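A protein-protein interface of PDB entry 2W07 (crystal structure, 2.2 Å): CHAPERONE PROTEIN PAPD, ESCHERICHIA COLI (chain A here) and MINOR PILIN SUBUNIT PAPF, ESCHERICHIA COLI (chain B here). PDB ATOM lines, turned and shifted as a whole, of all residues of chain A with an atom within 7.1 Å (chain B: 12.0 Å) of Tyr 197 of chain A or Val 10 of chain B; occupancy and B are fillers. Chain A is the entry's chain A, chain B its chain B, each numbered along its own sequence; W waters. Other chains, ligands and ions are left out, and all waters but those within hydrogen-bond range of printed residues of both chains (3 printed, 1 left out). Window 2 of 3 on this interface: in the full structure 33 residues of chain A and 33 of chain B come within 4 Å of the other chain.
Of the 11 printed residues of chain B, 8 touch a printed residue of chain A. Hydrophobic or aromatic side chains of chain B that line the printed part of chain A: Val 10, Tyr 11, Ile 12, Pro 13, Pro 14, Tyr 52 and Tyr 147. Of the 15 printed residues of chain A, 8 touch a printed residue of chain B. Along chain A the printed residues that touch a printed residue of chain B span positions 5 to 200. Among the printed residues, 16 pairs touch across the chains. Among the printed residues, no Asp or Glu carboxylate lies within 4 Å of a Lys or Arg side-chain nitrogen of the other chain.
Tyr 197 of chain A touches just these residues of chain B: Val 10, Tyr 11 and Ile 12. No residue of chain B comes within 4 Å of Pro 124 of chain A. No residue of chain B comes within 4 Å of Asn 195 of chain A. Of chain B, only Ile 12 comes within 4 Å of Gly 198 of chain A. Of the printed residues of chain A, Tyr 52 of chain B touches Arg 200 (3.7 Å). Of the printed residues of chain B, Asp 5 of chain A touches Tyr 11 (3.4 Å) and Pro 13 (3.7 Å). Printed residues of chain A within 4 Å of Ile 12 of chain B: Arg 6 (3.6 Å), Thr 7 (3.6 Å), Tyr 197 (2.9 Å) and Gly 198 (3.7 Å). Printed residues of chain B within 4 Å of Arg 6 of chain A: Tyr 11 (3.5 Å), Ile 12 (3.6 Å) and Pro 14 (3.8 Å). Of the printed residues of chain A, Asn 148 of chain B touches Arg 8 (2.6 Å) and Ile 194 (3.7 Å). The nearest residue of chain A that does not touch Val 10 of chain B is Gly 198 of chain A (6.0 Å). The nearest printed residue of chain A that does not touch Pro 13 of chain B is Arg 6 of chain A (4.3 Å).
The chain-end carboxylate (OXT) of Asn 148 of chain B lies within salt-bridge range of the guanidinium group (NH2) of Arg 8 of chain A, at 2.6 Å. N of Ile 12 of chain B lies within hydrogen-bond range of O of Tyr 197 of chain A (2.9 Å).
Water W2 lies within hydrogen-bond range of the side-chain hydroxyl of Thr 7 of chain A (2.6 Å), the backbone carbonyl oxygen of Ile 12 of chain B (2.7 Å) and the backbone carbonyl oxygen of Tyr 197 of chain A (3.1 Å). Water W3 lies within hydrogen-bond range of O of Asp 5 of chain A (2.8 Å) and O of Tyr 11 of chain B (2.8 Å). Water W1 lies within hydrogen-bond range of the backbone carbonyl oxygen (O) of Val 10 of chain A (3.2 Å) and the side-chain hydroxyl (OH) of Tyr 11 of chain B (3.3 Å).
The side-chain carboxylate of Asp 5 of chain A lies within salt-bridge range of the guanidinium group of Arg 6 of chain A (2.7 Å). The side-chain hydroxyl (OG1) of Thr 7 of chain A is in hydrogen-bond range of the guanidinium group (NH1) of Arg 8 of chain A (3.3 Å). The guanidinium group of Arg 8 of chain A lies close to the backbone carbonyl oxygen of Asn 195 of chain A, 3.4 Å away. The side-chain amide oxygen (OD1) of Asn 195 of chain A is in hydrogen-bond range of the backbone NH (N) of Tyr 197 of chain A (3.0 Å). N of Gly 198 of chain A lies within hydrogen-bond range of OD1 of Asn 195 of chain A, 3.1 Å away. The backbone NH (N) of Cys 15 of chain B lies within hydrogen-bond range of the side-chain hydroxyl (OH) of Tyr 147 of chain B (2.7 Å).
Among the printed residues, pairs that only touch across the chains: Tyr 197 of chain A with Val 10 of chain B (3.3 Å), Asp 5 of chain A with Tyr 11 of chain B (3.4 Å), Arg 6 of chain A with Tyr 11 of chain B (3.5 Å), Tyr 197 of chain A with Tyr 11 of chain B (3.6 Å), Thr 7 of chain A with Ile 12 of chain B (3.6 Å), Arg 6 of chain A with Ile 12 of chain B (3.6 Å), Ile 194 of chain A with Asn 148 of chain B (3.7 Å), Arg 200 of chain A with Tyr 52 of chain B (3.7 Å), Asp 5 of chain A with Pro 13 of chain B (3.7 Å), Gly 198 of chain A with Ile 12 of chain B (3.7 Å), Thr 7 of chain A with Pro 14 of chain B (3.8 Å), Thr 7 of chain A with Pro 13 of chain B (3.8 Å), Arg 6 of chain A with Pro 14 of chain B (3.8 Å) and Thr 7 of chain A with Tyr 147 of chain B (3.9 Å).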
ATOM      1  N   ASP A   5      16.046 -11.663   3.408  1.00  0.00           N
ATOM      2  CA  ASP A   5      15.883 -10.263   3.046  1.00  0.00           C
ATOM      3  C   ASP A   5      14.921 -10.022   1.871  1.00  0.00           C
ATOM      4  O   ASP A   5      14.591  -8.866   1.573  1.00  0.00           O
ATOM      5  CB  ASP A   5      17.258  -9.647   2.727  1.00  0.00           C
ATOM      6  CG  ASP A   5      17.995 -10.383   1.606  1.00  0.00           C
ATOM      7  OD1 ASP A   5      17.435 -11.356   1.053  1.00  0.00           O
ATOM      8  OD2 ASP A   5      19.135  -9.984   1.277  1.00  0.00           O
ATOM      9  N   ARG A   6      14.455 -11.093   1.223  1.00  0.00           N
ATOM     10  CA  ARG A   6      13.553 -10.953   0.062  1.00  0.00           C
ATOM     11  C   ARG A   6      12.597 -12.133  -0.163  1.00  0.00           C
ATOM     12  O   ARG A   6      12.785 -13.214   0.401  1.00  0.00           O
ATOM     13  CB  ARG A   6      14.393 -10.725  -1.202  1.00  0.00           C
ATOM     14  CG  ARG A   6      15.235 -11.932  -1.607  1.00  0.00           C
ATOM     15  CD  ARG A   6      16.429 -11.525  -2.449  1.00  0.00           C
ATOM     16  NE  ARG A   6      17.512 -10.971  -1.642  1.00  0.00           N
ATOM     17  CZ  ARG A   6      18.669 -10.547  -2.142  1.00  0.00           C
ATOM     18  NH1 ARG A   6      18.899 -10.607  -3.449  1.00  0.00           N
ATOM     19  NH2 ARG A   6      19.599 -10.061  -1.334  1.00  0.00           N
ATOM     20  N   THR A   7      11.581 -11.927  -1.000  1.00  0.00           N
ATOM     21  CA  THR A   7      10.579 -12.965  -1.282  1.00  0.00           C
ATOM     22  C   THR A   7      10.835 -13.750  -2.580  1.00  0.00           C
ATOM     23  O   THR A   7      10.129 -14.717  -2.893  1.00  0.00           O
ATOM     24  CB  THR A   7       9.146 -12.351  -1.335  1.00  0.00           C
ATOM     25  OG1 THR A   7       9.079 -11.360  -2.367  1.00  0.00           O
ATOM     26  CG2 THR A   7       8.802 -11.675   0.011  1.00  0.00           C
ATOM     27  N   ARG A   8      11.856 -13.329  -3.316  1.00  0.00           N
ATOM     28  CA  ARG A   8      12.251 -13.952  -4.582  1.00  0.00           C
ATOM     29  C   ARG A   8      13.687 -13.529  -4.826  1.00  0.00           C
ATOM     30  O   ARG A   8      14.093 -12.440  -4.425  1.00  0.00           O
ATOM     31  CB  ARG A   8      11.386 -13.422  -5.724  1.00  0.00           C
ATOM     32  CG  ARG A   8      10.948 -11.992  -5.454  1.00  0.00           C
ATOM     33  CD  ARG A   8      10.171 -11.345  -6.558  1.00  0.00           C
ATOM     34  NE  ARG A   8       9.108 -12.155  -7.144  1.00  0.00           N
ATOM     35  CZ  ARG A   8       8.183 -12.835  -6.476  1.00  0.00           C
ATOM     36  NH1 ARG A   8       8.153 -12.840  -5.147  1.00  0.00           N
ATOM     37  NH2 ARG A   8       7.269 -13.503  -7.159  1.00  0.00           N
ATOM     38  N   VAL A  10      16.756 -13.259  -7.874  1.00  0.00           N
ATOM     39  CA  VAL A  10      17.034 -13.291  -9.303  1.00  0.00           C
ATOM     40  C   VAL A  10      18.540 -13.463  -9.483  1.00  0.00           C
ATOM     41  O   VAL A  10      19.308 -12.561  -9.156  1.00  0.00           O
ATOM     42  CB  VAL A  10      16.583 -11.981  -9.987  1.00  0.00           C
ATOM     43  CG1 VAL A  10      16.950 -12.005 -11.466  1.00  0.00           C
ATOM     44  CG2 VAL A  10      15.081 -11.795  -9.811  1.00  0.00           C
ATOM     45  N   ARG A 123      17.613  -4.511 -17.948  1.00  0.00           N
ATOM     46  CA  ARG A 123      18.115  -3.218 -17.502  1.00  0.00           C
ATOM     47  C   ARG A 123      17.488  -2.957 -16.130  1.00  0.00           C
ATOM     48  O   ARG A 123      16.536  -3.631 -15.735  1.00  0.00           O
ATOM     49  CB  ARG A 123      17.703  -2.121 -18.483  1.00  0.00           C
ATOM     50  CG  ARG A 123      18.339  -2.239 -19.860  1.00  0.00           C
ATOM     51  CD  ARG A 123      17.615  -1.343 -20.849  1.00  0.00           C
ATOM     52  NE  ARG A 123      16.229  -1.768 -21.020  1.00  0.00           N
ATOM     53  CZ  ARG A 123      15.288  -1.048 -21.619  1.00  0.00           C
ATOM     54  NH1 ARG A 123      15.577   0.150 -22.112  1.00  0.00           N
ATOM     55  NH2 ARG A 123      14.054  -1.528 -21.728  1.00  0.00           N
ATOM     56  N   PRO A 124      18.016  -1.975 -15.385  1.00  0.00           N
ATOM     57  CA  PRO A 124      17.492  -1.649 -14.053  1.00  0.00           C
ATOM     58  C   PRO A 124      16.044  -1.148 -14.022  1.00  0.00           C
ATOM     59  O   PRO A 124      15.294  -1.441 -13.090  1.00  0.00           O
ATOM     60  CB  PRO A 124      18.474  -0.589 -13.551  1.00  0.00           C
ATOM     61  CG  PRO A 124      19.752  -0.946 -14.257  1.00  0.00           C
ATOM     62  CD  PRO A 124      19.259  -1.230 -15.649  1.00  0.00           C
ATOM     63  N   ASN A 125      15.655  -0.394 -15.044  1.00  0.00           N
ATOM     64  CA  ASN A 125      14.309   0.166 -15.115  1.00  0.00           C
ATOM     65  C   ASN A 125      13.371  -0.571 -16.076  1.00  0.00           C
ATOM     66  O   ASN A 125      12.260  -0.117 -16.341  1.00  0.00           O
ATOM     67  CB  ASN A 125      14.410   1.643 -15.516  1.00  0.00           C
ATOM     68  CG  ASN A 125      15.380   1.873 -16.680  1.00  0.00           C
ATOM     69  OD1 ASN A 125      15.196   1.336 -17.780  1.00  0.00           O
ATOM     70  ND2 ASN A 125      16.420   2.675 -16.437  1.00  0.00           N
ATOM     71  N   ILE A 194       4.001  -9.323  -9.063  1.00  0.00           N
ATOM     72  CA  ILE A 194       5.127  -9.146  -8.146  1.00  0.00           C
ATOM     73  C   ILE A 194       6.389  -9.037  -9.004  1.00  0.00           C
ATOM     74  O   ILE A 194       6.696  -9.960  -9.768  1.00  0.00           O
ATOM     75  CB  ILE A 194       5.302 -10.355  -7.194  1.00  0.00           C
ATOM     76  CG1 ILE A 194       4.004 -10.641  -6.434  1.00  0.00           C
ATOM     77  CG2 ILE A 194       6.423 -10.069  -6.195  1.00  0.00           C
ATOM     78  CD1 ILE A 194       4.048 -11.945  -5.650  1.00  0.00           C
ATOM     79  N   ASN A 195       7.114  -7.922  -8.902  1.00  0.00           N
ATOM     80  CA  ASN A 195       8.333  -7.756  -9.695  1.00  0.00           C
ATOM     81  C   ASN A 195       9.568  -8.318  -9.002  1.00  0.00           C
ATOM     82  O   ASN A 195       9.468  -8.899  -7.916  1.00  0.00           O
ATOM     83  CB  ASN A 195       8.573  -6.280 -10.075  1.00  0.00           C
ATOM     84  CG  ASN A 195       8.762  -5.356  -8.870  1.00  0.00           C
ATOM     85  OD1 ASN A 195       9.157  -5.778  -7.782  1.00  0.00           O
ATOM     86  ND2 ASN A 195       8.500  -4.068  -9.083  1.00  0.00           N
ATOM     87  N   ASP A 196      10.731  -8.139  -9.632  1.00  0.00           N
ATOM     88  CA  ASP A 196      11.990  -8.658  -9.108  1.00  0.00           C
ATOM     89  C   ASP A 196      12.290  -8.277  -7.664  1.00  0.00           C
ATOM     90  O   ASP A 196      12.958  -9.025  -6.944  1.00  0.00           O
ATOM     91  CB  ASP A 196      13.174  -8.196  -9.971  1.00  0.00           C
ATOM     92  CG  ASP A 196      13.179  -8.807 -11.369  1.00  0.00           C
ATOM     93  OD1 ASP A 196      12.403  -9.745 -11.646  1.00  0.00           O
ATOM     94  OD2 ASP A 196      13.984  -8.347 -12.196  1.00  0.00           O
ATOM     95  N   TYR A 197      11.808  -7.114  -7.240  1.00  0.00           N
ATOM     96  CA  TYR A 197      12.083  -6.646  -5.887  1.00  0.00           C
ATOM     97  C   TYR A 197      11.020  -6.969  -4.846  1.00  0.00           C
ATOM     98  O   TYR A 197      11.233  -6.749  -3.659  1.00  0.00           O
ATOM     99  CB  TYR A 197      12.336  -5.133  -5.908  1.00  0.00           C
ATOM    100  CG  TYR A 197      13.418  -4.733  -6.884  1.00  0.00           C
ATOM    101  CD1 TYR A 197      13.100  -4.215  -8.143  1.00  0.00           C
ATOM    102  CD2 TYR A 197      14.760  -4.910  -6.565  1.00  0.00           C
ATOM    103  CE1 TYR A 197      14.109  -3.880  -9.061  1.00  0.00           C
ATOM    104  CE2 TYR A 197      15.771  -4.583  -7.471  1.00  0.00           C
ATOM    105  CZ  TYR A 197      15.441  -4.069  -8.711  1.00  0.00           C
ATOM    106  OH  TYR A 197      16.453  -3.746  -9.588  1.00  0.00           O
ATOM    107  N   GLY A 198       9.881  -7.501  -5.273  1.00  0.00           N
ATOM    108  CA  GLY A 198       8.838  -7.801  -4.314  1.00  0.00           C
ATOM    109  C   GLY A 198       7.795  -6.696  -4.322  1.00  0.00           C
ATOM    110  O   GLY A 198       6.833  -6.719  -3.552  1.00  0.00           O
ATOM    111  N   GLY A 199       7.999  -5.713  -5.194  1.00  0.00           N
ATOM    112  CA  GLY A 199       7.035  -4.637  -5.316  1.00  0.00           C
ATOM    113  C   GLY A 199       5.853  -5.245  -6.048  1.00  0.00           C
ATOM    114  O   GLY A 199       6.000  -6.281  -6.701  1.00  0.00           O
ATOM    115  N   ARG A 200       4.683  -4.623  -5.942  1.00  0.00           N
ATOM    116  CA  ARG A 200       3.494  -5.145  -6.603  1.00  0.00           C
ATOM    117  C   ARG A 200       2.871  -4.065  -7.466  1.00  0.00           C
ATOM    118  O   ARG A 200       1.898  -3.414  -7.073  1.00  0.00           O
ATOM    119  CB  ARG A 200       2.496  -5.646  -5.559  1.00  0.00           C
ATOM    120  CG  ARG A 200       3.105  -6.664  -4.607  1.00  0.00           C
ATOM    121  CD  ARG A 200       2.354  -6.709  -3.286  1.00  0.00           C
ATOM    122  NE  ARG A 200       1.363  -7.773  -3.232  1.00  0.00           N
ATOM    123  CZ  ARG A 200       1.642  -9.050  -2.997  1.00  0.00           C
ATOM    124  NH1 ARG A 200       2.890  -9.441  -2.787  1.00  0.00           N
ATOM    125  NH2 ARG A 200       0.663  -9.938  -2.962  1.00  0.00           N
ATOM    126  N   ASN B   9      14.627  -1.719   3.072  1.00  0.00           N
ATOM    127  CA  ASN B   9      15.633  -1.978   1.998  1.00  0.00           C
ATOM    128  C   ASN B   9      14.949  -2.052   0.641  1.00  0.00           C
ATOM    129  O   ASN B   9      13.722  -2.024   0.558  1.00  0.00           O
ATOM    130  CB  ASN B   9      16.377  -3.279   2.277  1.00  0.00           C
ATOM    131  N   VAL B  10      15.747  -2.143  -0.422  1.00  0.00           N
ATOM    132  CA  VAL B  10      15.203  -2.223  -1.777  1.00  0.00           C
ATOM    133  C   VAL B  10      14.317  -3.448  -1.964  1.00  0.00           C
ATOM    134  O   VAL B  10      13.308  -3.376  -2.667  1.00  0.00           O
ATOM    135  CB  VAL B  10      16.326  -2.242  -2.848  1.00  0.00           C
ATOM    136  CG1 VAL B  10      15.850  -2.960  -4.108  1.00  0.00           C
ATOM    137  CG2 VAL B  10      16.721  -0.814  -3.205  1.00  0.00           C
ATOM    138  N   TYR B  11      14.682  -4.571  -1.344  1.00  0.00           N
ATOM    139  CA  TYR B  11      13.871  -5.782  -1.473  1.00  0.00           C
ATOM    140  C   TYR B  11      12.789  -5.840  -0.415  1.00  0.00           C
ATOM    141  O   TYR B  11      13.063  -5.667   0.772  1.00  0.00           O
ATOM    142  CB  TYR B  11      14.720  -7.051  -1.353  1.00  0.00           C
ATOM    143  CG  TYR B  11      15.833  -7.158  -2.356  1.00  0.00           C
ATOM    144  CD1 TYR B  11      17.138  -6.819  -2.010  1.00  0.00           C
ATOM    145  CD2 TYR B  11      15.582  -7.584  -3.658  1.00  0.00           C
ATOM    146  CE1 TYR B  11      18.170  -6.903  -2.936  1.00  0.00           C
ATOM    147  CE2 TYR B  11      16.603  -7.671  -4.593  1.00  0.00           C
ATOM    148  CZ  TYR B  11      17.897  -7.329  -4.226  1.00  0.00           C
ATOM    149  OH  TYR B  11      18.911  -7.414  -5.152  1.00  0.00           O
ATOM    150  N   ILE B  12      11.554  -6.068  -0.846  1.00  0.00           N
ATOM    151  CA  ILE B  12      10.458  -6.188   0.096  1.00  0.00           C
ATOM    152  C   ILE B  12      10.707  -7.526   0.785  1.00  0.00           C
ATOM    153  O   ILE B  12      10.801  -8.558   0.128  1.00  0.00           O
ATOM    154  CB  ILE B  12       9.094  -6.190  -0.617  1.00  0.00           C
ATOM    155  CG1 ILE B  12       8.649  -4.748  -0.886  1.00  0.00           C
ATOM    156  CG2 ILE B  12       8.062  -6.898   0.230  1.00  0.00           C
ATOM    157  CD1 ILE B  12       9.497  -4.004  -1.889  1.00  0.00           C
ATOM    158  N   PRO B  13      10.831  -7.520   2.120  1.00  0.00           N
ATOM    159  CA  PRO B  13      11.084  -8.751   2.871  1.00  0.00           C
ATOM    160  C   PRO B  13       9.877  -9.634   3.108  1.00  0.00           C
ATOM    161  O   PRO B  13       8.738  -9.222   2.911  1.00  0.00           O
ATOM    162  CB  PRO B  13      11.675  -8.227   4.179  1.00  0.00           C
ATOM    163  CG  PRO B  13      10.868  -6.998   4.402  1.00  0.00           C
ATOM    164  CD  PRO B  13      10.829  -6.352   3.022  1.00  0.00           C
ATOM    165  N   PRO B  14      10.120 -10.882   3.529  1.00  0.00           N
ATOM    166  CA  PRO B  14       9.022 -11.808   3.796  1.00  0.00           C
ATOM    167  C   PRO B  14       8.390 -11.458   5.135  1.00  0.00           C
ATOM    168  O   PRO B  14       8.943 -10.679   5.910  1.00  0.00           O
ATOM    169  CB  PRO B  14       9.714 -13.167   3.801  1.00  0.00           C
ATOM    170  CG  PRO B  14      11.069 -12.849   4.296  1.00  0.00           C
ATOM    171  CD  PRO B  14      11.416 -11.578   3.569  1.00  0.00           C
ATOM    172  N   CYS B  15       7.234 -12.037   5.406  1.00  0.00           N
ATOM    173  CA  CYS B  15       6.531 -11.760   6.644  1.00  0.00           C
ATOM    174  C   CYS B  15       7.256 -12.288   7.879  1.00  0.00           C
ATOM    175  O   CYS B  15       8.005 -13.264   7.814  1.00  0.00           O
ATOM    176  CB  CYS B  15       5.135 -12.357   6.562  1.00  0.00           C
ATOM    177  SG  CYS B  15       4.386 -12.139   4.917  1.00  0.00           S
ATOM    178  N   PRO B  51       4.752  -7.147   4.949  1.00  0.00           N
ATOM    179  CA  PRO B  51       5.127  -5.817   4.450  1.00  0.00           C
ATOM    180  C   PRO B  51       4.107  -5.186   3.498  1.00  0.00           C
ATOM    181  O   PRO B  51       3.943  -3.962   3.473  1.00  0.00           O
ATOM    182  CB  PRO B  51       6.460  -6.072   3.738  1.00  0.00           C
ATOM    183  CG  PRO B  51       6.980  -7.317   4.389  1.00  0.00           C
ATOM    184  CD  PRO B  51       5.736  -8.146   4.499  1.00  0.00           C
ATOM    185  N   TYR B  52       3.439  -6.025   2.710  1.00  0.00           N
ATOM    186  CA  TYR B  52       2.448  -5.551   1.748  1.00  0.00           C
ATOM    187  C   TYR B  52       1.032  -5.928   2.166  1.00  0.00           C
ATOM    188  O   TYR B  52       0.710  -7.105   2.301  1.00  0.00           O
ATOM    189  CB  TYR B  52       2.755  -6.120   0.357  1.00  0.00           C
ATOM    190  N   TYR B 147       6.498 -18.531  -0.420  1.00  0.00           N
ATOM    191  CA  TYR B 147       6.098 -17.283  -1.054  1.00  0.00           C
ATOM    192  C   TYR B 147       5.865 -17.316  -2.556  1.00  0.00           C
ATOM    193  O   TYR B 147       6.571 -17.991  -3.302  1.00  0.00           O
ATOM    194  CB  TYR B 147       7.127 -16.192  -0.748  1.00  0.00           C
ATOM    195  CG  TYR B 147       7.096 -15.733   0.685  1.00  0.00           C
ATOM    196  CD1 TYR B 147       7.653 -16.509   1.698  1.00  0.00           C
ATOM    197  CD2 TYR B 147       6.444 -14.552   1.038  1.00  0.00           C
ATOM    198  CE1 TYR B 147       7.555 -16.123   3.029  1.00  0.00           C
ATOM    199  CE2 TYR B 147       6.337 -14.160   2.364  1.00  0.00           C
ATOM    200  CZ  TYR B 147       6.891 -14.949   3.353  1.00  0.00           C
ATOM    201  OH  TYR B 147       6.750 -14.577   4.666  1.00  0.00           O
ATOM    202  N   ASN B 148       4.862 -16.558  -2.984  1.00  0.00           N
ATOM    203  CA  ASN B 148       4.546 -16.433  -4.390  1.00  0.00           C
ATOM    204  C   ASN B 148       5.521 -15.403  -4.924  1.00  0.00           C
ATOM    205  O   ASN B 148       6.185 -14.777  -4.076  1.00  0.00           O
ATOM    206  CB  ASN B 148       3.118 -15.939  -4.570  1.00  0.00           C
ATOM    207  CG  ASN B 148       2.096 -16.982  -4.176  1.00  0.00           C
ATOM    208  OD1 ASN B 148       2.137 -18.111  -4.660  1.00  0.00           O
ATOM    209  ND2 ASN B 148       1.174 -16.610  -3.300  1.00  0.00           N
ATOM    210  OXT ASN B 148       5.616 -15.237  -6.158  1.00  0.00           O
HETATM  211  O   HOH W   1      19.341  -9.844  -7.413  1.00  0.00           O
HETATM  212  O   HOH W   2      10.868  -9.519  -2.418  1.00  0.00           O
HETATM  213  O   HOH W   3      14.652  -6.456   2.956  1.00  0.00           O
